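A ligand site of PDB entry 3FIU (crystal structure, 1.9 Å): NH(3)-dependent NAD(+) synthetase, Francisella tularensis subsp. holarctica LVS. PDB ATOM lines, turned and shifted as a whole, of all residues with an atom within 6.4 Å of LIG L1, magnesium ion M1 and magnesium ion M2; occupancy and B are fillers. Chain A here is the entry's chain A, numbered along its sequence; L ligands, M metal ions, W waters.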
ATOM      1  N   GLY A  35      -5.347  19.488  -1.047  1.00  0.00           N
ATOM      2  CA  GLY A  35      -5.576  18.416  -0.066  1.00  0.00           C
ATOM      3  C   GLY A  35      -6.990  18.534   0.507  1.00  0.00           C
ATOM      4  O   GLY A  35      -7.392  19.605   1.002  1.00  0.00           O
ATOM      5  N   LEU A  36      -7.758  17.440   0.424  1.00  0.00           N
ATOM      6  CA  LEU A  36      -9.143  17.433   0.930  1.00  0.00           C
ATOM      7  C   LEU A  36      -9.256  16.664   2.227  1.00  0.00           C
ATOM      8  O   LEU A  36      -9.086  15.440   2.258  1.00  0.00           O
ATOM      9  CB  LEU A  36     -10.119  16.828  -0.089  1.00  0.00           C
ATOM     10  CG  LEU A  36     -10.744  17.619  -1.216  1.00  0.00           C
ATOM     11  CD1 LEU A  36     -11.832  16.720  -1.800  1.00  0.00           C
ATOM     12  CD2 LEU A  36     -11.372  18.916  -0.759  1.00  0.00           C
ATOM     13  N   SER A  37      -9.557  17.384   3.305  1.00  0.00           N
ATOM     14  CA  SER A  37      -9.612  16.812   4.639  1.00  0.00           C
ATOM     15  C   SER A  37     -11.013  16.311   5.004  1.00  0.00           C
ATOM     16  O   SER A  37     -11.169  15.593   5.963  1.00  0.00           O
ATOM     17  CB  SER A  37      -9.232  17.885   5.643  1.00  0.00           C
ATOM     18  OG  SER A  37     -10.172  18.951   5.544  1.00  0.00           O
ATOM     19  N   GLY A  38     -12.026  16.708   4.247  1.00  0.00           N
ATOM     20  CA  GLY A  38     -13.416  16.417   4.591  1.00  0.00           C
ATOM     21  C   GLY A  38     -14.008  17.589   5.358  1.00  0.00           C
ATOM     22  O   GLY A  38     -15.215  17.597   5.675  1.00  0.00           O
ATOM     23  N   GLY A  39     -13.159  18.601   5.616  1.00  0.00           N
ATOM     24  CA  GLY A  39     -13.611  19.889   6.229  1.00  0.00           C
ATOM     25  C   GLY A  39     -14.139  20.896   5.210  1.00  0.00           C
ATOM     26  O   GLY A  39     -14.001  20.729   4.008  1.00  0.00           O
ATOM     27  N   ILE A  40     -14.734  21.987   5.720  1.00  0.00           N
ATOM     28  CA  ILE A  40     -15.353  23.002   4.873  1.00  0.00           C
ATOM     29  C   ILE A  40     -14.375  23.877   4.060  1.00  0.00           C
ATOM     30  O   ILE A  40     -14.671  24.234   2.919  1.00  0.00           O
ATOM     31  CB  ILE A  40     -16.239  23.945   5.746  1.00  0.00           C
ATOM     32  CG1 ILE A  40     -17.085  24.844   4.850  1.00  0.00           C
ATOM     33  CG2 ILE A  40     -15.372  24.831   6.705  1.00  0.00           C
ATOM     34  CD1 ILE A  40     -18.097  24.094   4.071  1.00  0.00           C
ATOM     35  N   ASP A  41     -13.211  24.227   4.637  1.00  0.00           N
ATOM     36  CA  ASP A  41     -12.272  25.159   3.945  1.00  0.00           C
ATOM     37  C   ASP A  41     -11.764  24.506   2.672  1.00  0.00           C
ATOM     38  O   ASP A  41     -11.788  25.115   1.606  1.00  0.00           O
ATOM     39  CB  ASP A  41     -11.049  25.526   4.820  1.00  0.00           C
ATOM     40  CG  ASP A  41     -11.411  26.260   6.109  1.00  0.00           C
ATOM     41  OD1 ASP A  41     -12.425  26.999   6.134  1.00  0.00           O
ATOM     42  OD2 ASP A  41     -10.637  26.088   7.096  1.00  0.00           O
ATOM     43  N   SER A  42     -11.314  23.254   2.787  1.00  0.00           N
ATOM     44  CA  SER A  42     -10.778  22.579   1.607  1.00  0.00           C
ATOM     45  C   SER A  42     -11.903  22.201   0.646  1.00  0.00           C
ATOM     46  O   SER A  42     -11.701  22.237  -0.580  1.00  0.00           O
ATOM     47  CB  SER A  42      -9.929  21.357   1.961  1.00  0.00           C
ATOM     48  OG  SER A  42     -10.648  20.470   2.818  1.00  0.00           O
ATOM     49  N   ALA A  43     -13.087  21.896   1.187  1.00  0.00           N
ATOM     50  CA  ALA A  43     -14.239  21.625   0.327  1.00  0.00           C
ATOM     51  C   ALA A  43     -14.573  22.841  -0.586  1.00  0.00           C
ATOM     52  O   ALA A  43     -14.762  22.714  -1.823  1.00  0.00           O
ATOM     53  CB  ALA A  43     -15.451  21.190   1.149  1.00  0.00           C
ATOM     54  N   THR A 142      -5.704  26.499   1.911  1.00  0.00           N
ATOM     55  CA  THR A 142      -7.116  26.651   2.284  1.00  0.00           C
ATOM     56  C   THR A 142      -7.351  27.595   3.472  1.00  0.00           C
ATOM     57  O   THR A 142      -8.483  27.738   3.927  1.00  0.00           O
ATOM     58  CB  THR A 142      -7.746  25.297   2.633  1.00  0.00           C
ATOM     59  OG1 THR A 142      -7.113  24.800   3.797  1.00  0.00           O
ATOM     60  CG2 THR A 142      -7.618  24.290   1.470  1.00  0.00           C
ATOM     61  N   ASP A 143      -6.270  28.196   3.978  1.00  0.00           N
ATOM     62  CA  ASP A 143      -6.332  29.147   5.143  1.00  0.00           C
ATOM     63  C   ASP A 143      -7.412  30.215   4.909  1.00  0.00           C
ATOM     64  O   ASP A 143      -7.444  30.864   3.858  1.00  0.00           O
ATOM     65  CB  ASP A 143      -4.981  29.813   5.380  1.00  0.00           C
ATOM     66  CG  ASP A 143      -3.832  28.808   5.463  1.00  0.00           C
ATOM     67  OD1 ASP A 143      -3.369  28.519   6.585  1.00  0.00           O
ATOM     68  OD2 ASP A 143      -3.425  28.266   4.404  1.00  0.00           O
ATOM     69  N   ASN A 144      -8.303  30.383   5.902  1.00  0.00           N
ATOM     70  CA  ASN A 144      -9.292  31.451   5.861  1.00  0.00           C
ATOM     71  C   ASN A 144      -8.776  32.585   6.776  1.00  0.00           C
ATOM     72  O   ASN A 144      -7.718  32.413   7.428  1.00  0.00           O
ATOM     73  CB  ASN A 144     -10.690  30.945   6.290  1.00  0.00           C
ATOM     74  CG  ASN A 144     -10.687  30.350   7.684  1.00  0.00           C
ATOM     75  OD1 ASN A 144     -10.212  30.962   8.629  1.00  0.00           O
ATOM     76  ND2 ASN A 144     -11.226  29.126   7.822  1.00  0.00           N
ATOM     77  N   GLU A 147      -8.125  31.374  10.629  1.00  0.00           N
ATOM     78  CA  GLU A 147      -6.896  30.589  10.774  1.00  0.00           C
ATOM     79  C   GLU A 147      -5.658  31.437  10.591  1.00  0.00           C
ATOM     80  O   GLU A 147      -4.712  31.351  11.392  1.00  0.00           O
ATOM     81  CB  GLU A 147      -6.902  29.418   9.801  1.00  0.00           C
ATOM     82  CG  GLU A 147      -8.145  28.595   9.918  1.00  0.00           C
ATOM     83  CD  GLU A 147      -8.303  27.583   8.777  1.00  0.00           C
ATOM     84  OE1 GLU A 147      -8.610  26.437   9.103  1.00  0.00           O
ATOM     85  OE2 GLU A 147      -8.086  27.916   7.599  1.00  0.00           O
ATOM     86  N   TYR A 152      -3.520  29.533  13.260  1.00  0.00           N
ATOM     87  CA  TYR A 152      -3.920  28.141  13.469  1.00  0.00           C
ATOM     88  C   TYR A 152      -3.657  27.362  12.175  1.00  0.00           C
ATOM     89  O   TYR A 152      -4.601  26.980  11.424  1.00  0.00           O
ATOM     90  CB  TYR A 152      -5.395  27.994  13.926  1.00  0.00           C
ATOM     91  CG  TYR A 152      -5.699  26.631  14.558  1.00  0.00           C
ATOM     92  CD1 TYR A 152      -6.860  26.415  15.319  1.00  0.00           C
ATOM     93  CD2 TYR A 152      -4.829  25.551  14.398  1.00  0.00           C
ATOM     94  CE1 TYR A 152      -7.134  25.158  15.891  1.00  0.00           C
ATOM     95  CE2 TYR A 152      -5.098  24.293  14.950  1.00  0.00           C
ATOM     96  CZ  TYR A 152      -6.247  24.098  15.703  1.00  0.00           C
ATOM     97  OH  TYR A 152      -6.482  22.841  16.245  1.00  0.00           O
ATOM     98  N   ASP A 158       0.278  23.145   6.193  1.00  0.00           N
ATOM     99  CA  ASP A 158      -0.910  23.669   5.503  1.00  0.00           C
ATOM    100  C   ASP A 158      -0.811  25.175   5.293  1.00  0.00           C
ATOM    101  O   ASP A 158      -1.481  25.713   4.428  1.00  0.00           O
ATOM    102  CB  ASP A 158      -2.214  23.262   6.234  1.00  0.00           C
ATOM    103  CG  ASP A 158      -2.255  23.762   7.662  1.00  0.00           C
ATOM    104  OD1 ASP A 158      -3.245  24.426   7.991  1.00  0.00           O
ATOM    105  OD2 ASP A 158      -1.305  23.503   8.424  1.00  0.00           O
ATOM    106  N   LYS A 171     -14.969  32.851   8.778  1.00  0.00           N
ATOM    107  CA  LYS A 171     -15.431  31.455   8.730  1.00  0.00           C
ATOM    108  C   LYS A 171     -16.898  31.358   8.268  1.00  0.00           C
ATOM    109  O   LYS A 171     -17.269  30.511   7.461  1.00  0.00           O
ATOM    110  CB  LYS A 171     -15.215  30.789  10.086  1.00  0.00           C
ATOM    111  CG  LYS A 171     -15.408  29.261  10.082  1.00  0.00           C
ATOM    112  CD  LYS A 171     -14.236  28.595   9.337  1.00  0.00           C
ATOM    113  CE  LYS A 171     -14.370  27.064   9.383  1.00  0.00           C
ATOM    114  NZ  LYS A 171     -13.113  26.394   8.778  1.00  0.00           N
ATOM    115  N   PHE A 175     -18.557  29.243   5.121  1.00  0.00           N
ATOM    116  CA  PHE A 175     -19.759  28.408   5.178  1.00  0.00           C
ATOM    117  C   PHE A 175     -20.837  28.864   4.189  1.00  0.00           C
ATOM    118  O   PHE A 175     -21.500  28.035   3.558  1.00  0.00           O
ATOM    119  CB  PHE A 175     -20.306  28.338   6.598  1.00  0.00           C
ATOM    120  CG  PHE A 175     -19.623  27.329   7.475  1.00  0.00           C
ATOM    121  CD1 PHE A 175     -18.912  27.746   8.594  1.00  0.00           C
ATOM    122  CD2 PHE A 175     -19.726  25.977   7.215  1.00  0.00           C
ATOM    123  CE1 PHE A 175     -18.291  26.822   9.447  1.00  0.00           C
ATOM    124  CE2 PHE A 175     -19.092  25.033   8.063  1.00  0.00           C
ATOM    125  CZ  PHE A 175     -18.379  25.470   9.172  1.00  0.00           C
ATOM    126  N   ALA A 191     -18.276  19.936  12.976  1.00  0.00           N
ATOM    127  CA  ALA A 191     -17.372  20.835  13.694  1.00  0.00           C
ATOM    128  C   ALA A 191     -16.035  21.002  12.946  1.00  0.00           C
ATOM    129  O   ALA A 191     -15.393  19.977  12.622  1.00  0.00           O
ATOM    130  CB  ALA A 191     -17.098  20.268  15.113  1.00  0.00           C
ATOM    131  N   PRO A 192     -15.611  22.258  12.657  1.00  0.00           N
ATOM    132  CA  PRO A 192     -14.235  22.518  12.186  1.00  0.00           C
ATOM    133  C   PRO A 192     -13.204  21.853  13.100  1.00  0.00           C
ATOM    134  O   PRO A 192     -13.300  21.933  14.330  1.00  0.00           O
ATOM    135  CB  PRO A 192     -14.136  24.047  12.266  1.00  0.00           C
ATOM    136  CG  PRO A 192     -15.539  24.509  11.976  1.00  0.00           C
ATOM    137  CD  PRO A 192     -16.389  23.507  12.740  1.00  0.00           C
ATOM    138  N   SER A 193     -12.227  21.157  12.499  1.00  0.00           N
ATOM    139  CA  SER A 193     -11.350  20.292  13.277  1.00  0.00           C
ATOM    140  C   SER A 193     -10.060  20.043  12.519  1.00  0.00           C
ATOM    141  O   SER A 193     -10.104  19.865  11.297  1.00  0.00           O
ATOM    142  CB  SER A 193     -12.038  18.960  13.566  1.00  0.00           C
ATOM    143  OG  SER A 193     -11.138  18.052  14.165  1.00  0.00           O
ATOM    144  N   ALA A 194      -8.934  19.989  13.226  1.00  0.00           N
ATOM    145  CA  ALA A 194      -7.667  19.657  12.571  1.00  0.00           C
ATOM    146  C   ALA A 194      -7.522  18.142  12.363  1.00  0.00           C
ATOM    147  O   ALA A 194      -6.542  17.697  11.757  1.00  0.00           O
ATOM    148  CB  ALA A 194      -6.440  20.249  13.371  1.00  0.00           C
ATOM    149  N   GLY A 195      -8.465  17.359  12.919  1.00  0.00           N
ATOM    150  CA  GLY A 195      -8.510  15.887  12.747  1.00  0.00           C
ATOM    151  C   GLY A 195      -7.464  15.037  13.479  1.00  0.00           C
ATOM    152  O   GLY A 195      -7.239  13.866  13.116  1.00  0.00           O
ATOM    153  N   ASP A 202     -11.767  22.754  16.550  1.00  0.00           N
ATOM    154  CA  ASP A 202     -11.002  23.990  16.529  1.00  0.00           C
ATOM    155  C   ASP A 202     -11.403  24.931  17.679  1.00  0.00           C
ATOM    156  O   ASP A 202     -10.547  25.560  18.307  1.00  0.00           O
ATOM    157  CB  ASP A 202     -11.252  24.739  15.231  1.00  0.00           C
ATOM    158  CG  ASP A 202     -10.640  24.035  14.013  1.00  0.00           C
ATOM    159  OD1 ASP A 202     -10.079  22.920  14.141  1.00  0.00           O
ATOM    160  OD2 ASP A 202     -10.760  24.626  12.919  1.00  0.00           O
ATOM    161  N   TYR A 210     -15.602  30.539  16.436  1.00  0.00           N
ATOM    162  CA  TYR A 210     -15.417  31.234  15.163  1.00  0.00           C
ATOM    163  C   TYR A 210     -16.253  32.497  15.082  1.00  0.00           C
ATOM    164  O   TYR A 210     -15.836  33.466  14.455  1.00  0.00           O
ATOM    165  CB  TYR A 210     -15.655  30.332  13.940  1.00  0.00           C
ATOM    166  CG  TYR A 210     -14.442  29.443  13.659  1.00  0.00           C
ATOM    167  CD1 TYR A 210     -14.458  28.070  13.979  1.00  0.00           C
ATOM    168  CD2 TYR A 210     -13.265  29.997  13.111  1.00  0.00           C
ATOM    169  CE1 TYR A 210     -13.314  27.251  13.736  1.00  0.00           C
ATOM    170  CE2 TYR A 210     -12.150  29.196  12.859  1.00  0.00           C
ATOM    171  CZ  TYR A 210     -12.184  27.841  13.162  1.00  0.00           C
ATOM    172  OH  TYR A 210     -11.053  27.078  12.881  1.00  0.00           O
HETATM  173  P1  LIG L   1     -10.583  22.069   6.536  1.00  0.00           P
HETATM  174  O1  LIG L   1     -11.067  21.802   5.128  1.00  0.00           O
HETATM  175  O2  LIG L   1      -9.498  23.105   6.547  1.00  0.00           O
HETATM  176  O3  LIG L   1     -10.091  20.827   7.267  1.00  0.00           O
HETATM  177  O4  LIG L   1     -11.818  22.728   7.357  1.00  0.00           O
HETATM  178  P2  LIG L   1     -11.709  23.107   8.919  1.00  0.00           P
HETATM  179  O5  LIG L   1     -10.648  24.185   9.109  1.00  0.00           O
HETATM  180  O6  LIG L   1     -13.078  23.674   9.175  1.00  0.00           O
HETATM  181  O7  LIG L   1     -11.463  21.914   9.805  1.00  0.00           O
HETATM  182  P1  LG2 L   2      -7.291  22.216   9.173  1.00  0.00           P
HETATM  183  O1  LG2 L   2      -7.604  23.678   8.961  1.00  0.00           O
HETATM  184  O2  LG2 L   2      -6.032  22.011  10.042  1.00  0.00           O
HETATM  185  O3  LG2 L   2      -8.397  21.289   9.535  1.00  0.00           O
HETATM  186  O4  LG2 L   2      -6.725  21.663   7.745  1.00  0.00           O
HETATM  187  C1  LG2 L   2      -5.841  22.497   6.980  1.00  0.00           C
HETATM  188  C2  LG2 L   2      -5.719  21.912   5.580  1.00  0.00           C
HETATM  189  O5  LG2 L   2      -4.865  20.763   5.566  1.00  0.00           O
HETATM  190  C3  LG2 L   2      -7.033  21.375   5.034  1.00  0.00           C
HETATM  191  O6  LG2 L   2      -7.797  22.468   4.525  1.00  0.00           O
HETATM  192  C4  LG2 L   2      -6.553  20.432   3.938  1.00  0.00           C
HETATM  193  O7  LG2 L   2      -6.279  21.145   2.711  1.00  0.00           O
HETATM  194  C5  LG2 L   2      -5.272  19.866   4.533  1.00  0.00           C
HETATM  195  N1  LG2 L   2      -5.572  18.563   5.173  1.00  0.00           N
HETATM  196  C6  LG2 L   2      -5.788  18.333   6.501  1.00  0.00           C
HETATM  197  N2  LG2 L   2      -6.053  17.020   6.725  1.00  0.00           N
HETATM  198  C7  LG2 L   2      -6.048  16.405   5.523  1.00  0.00           C
HETATM  199  C8  LG2 L   2      -6.241  15.020   5.041  1.00  0.00           C
HETATM  200  N3  LG2 L   2      -6.560  14.036   5.917  1.00  0.00           N
HETATM  201  N4  LG2 L   2      -6.108  14.834   3.714  1.00  0.00           N
HETATM  202  C9  LG2 L   2      -5.825  15.805   2.829  1.00  0.00           C
HETATM  203  N5  LG2 L   2      -5.611  17.101   3.187  1.00  0.00           N
HETATM  204  C10 LG2 L   2      -5.710  17.419   4.505  1.00  0.00           C
HETATM  205 MG    MG M   1      -9.188  24.738   7.830  1.00  0.00          MG
HETATM  206 MG    MG M   2     -10.116  20.413   9.184  1.00  0.00          MG
HETATM  207  O   HOH W   1      -8.801  18.765   8.896  1.00  0.00           O
HETATM  208  O   HOH W   2      -7.708  25.612   6.391  1.00  0.00           O
HETATM  209  O   HOH W   3     -14.941  21.920   8.617  1.00  0.00           O
HETATM  210  O   HOH W   4     -14.044  19.664  10.102  1.00  0.00           O
HETATM  211  O   HOH W   5     -10.976  27.363  10.163  1.00  0.00           O
HETATM  212  O   HOH W   6     -11.613  19.050   9.135  1.00  0.00           O
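The backbone NH of Ser 42 sits at hydrogen-bond distance from an oxygen (O1) of LIG L1, at 2.8 Å.
O7 of LG2 L2 sits at hydrogen-bond distance from O of Gly 35 (2.6 Å).
The side-chain hydroxyl of Ser 42 sits at hydrogen-bond distance from an oxygen (O1) of LIG L1, at 2.7 Å.
An oxygen (O7) of LIG L1 sits close to the backbone NH of Ser 193, 2.9 Å away.
OG of Ser 37 is in hydrogen-bond range of O1 of LIG L1, at 3.0 Å.
The side-chain amino group of Lys 171 is in salt-bridge range of an oxygen (O6) of LIG L1 (2.7 Å).
O6 of LG2 L2 lies within hydrogen-bond range of OG1 of Thr 142, at 2.5 Å.
O4 of LIG L1 is in hydrogen-bond range of N of Ile 40.
The backbone NH (N) of Asp 41 lies within hydrogen-bond range of an oxygen (O1) of LIG L1 (3.3 Å).
The side-chain amino group (NZ) of Lys 171 sits close to the side-chain amide nitrogen (ND2) of Asn 144.
The side-chain hydroxyl (OG) of Ser 193 lies within hydrogen-bond range of the backbone NH (N) of Gly 195.
The backbone carbonyl oxygen (O) of Glu 147 lies within hydrogen-bond range of the backbone NH (N) of Tyr 152, at 2.9 Å.
OD1 of Asp 41 lies within salt-bridge range of NZ of Lys 171 (2.8 Å).
The side-chain carboxylate (OD2) of Asp 202 sits at hydrogen-bond distance from the side-chain hydroxyl (OH) of Tyr 210 (2.5 Å).
The side-chain hydroxyl (OG) of Ser 37 is in hydrogen-bond range of the side-chain hydroxyl (OG) of Ser 42 (3.2 Å).
The side-chain carboxylate (OD1) of Asp 41 sits at hydrogen-bond distance from the side-chain amide nitrogen (ND2) of Asn 144 (3.0 Å).
The backbone NH (N) of Ser 193 sits close to the side-chain carboxylate (OD1) of Asp 202 (3.2 Å).
O of Gly 39 sits close to O1 of LIG L1, 3.3 Å away.
Residues that only touch LIG L1: Pro 192 and Asp 202.
Ten residues have an atom within 4 Å of LIG L1: Ser 37, Gly 39, Ile 40, Asp 41, Ser 42, Glu 147, Lys 171, Pro 192, Ser 193 and Asp 202.
The nearest printed residue that does not touch LIG L1 is Thr 142 (4.02 Å).
Of the 24 residues printed, 2 come within 4 Å of magnesium ion M1.
The nearest printed residue that does not touch magnesium ion M1 is Lys 171 (4.4 Å).
Residues that only touch magnesium ion M2: Ser 37 (3.9 Å).
Of the 24 residues printed, 2 come within 4 Å of magnesium ion M2.
The nearest printed residue that does not touch magnesium ion M2 is Ala 194 (4.2 Å).
Magnesium ion M1 is bound by O5 of LIG L1 (2.0 Å), O2 of LIG L1 (2.1 Å), OD2 of Asp 41 (2.1 Å), OE1 of Glu 147 (2.2 Å), O1 of LG2 L2 (2.2 Å) and water W2 (2.2 Å).
Magnesium ion M1 has six donor atoms within binding distance.
Magnesium ion M2 is bound by an oxygen (O3) of LG2 L2 (2.0 Å), an oxygen (O3) of LIG L1 (2.0 Å), water W6 (2.0 Å), an oxygen (O7) of LIG L1 (2.1 Å), water W1 (2.1 Å) and the backbone carbonyl oxygen (O) of Ser 193 (2.2 Å).
Magnesium ion M2 has six donor atoms within binding distance.
Water W2 bridges the side-chain carboxylate (OE2) of Glu 147 (2.6 Å) and the side-chain hydroxyl (OG1) of Thr 142 (2.8 Å).
Water W3 lies within hydrogen-bond range of O6 of LIG L1 (2.6 Å) and N of Ile 40 (2.9 Å).
Water W5 lies within hydrogen-bond range of the side-chain amino group (NZ) of Lys 171 (2.7 Å), the side-chain hydroxyl (OH) of Tyr 210 (2.7 Å) and the side-chain amide nitrogen (ND2) of Asn 144 (2.9 Å).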
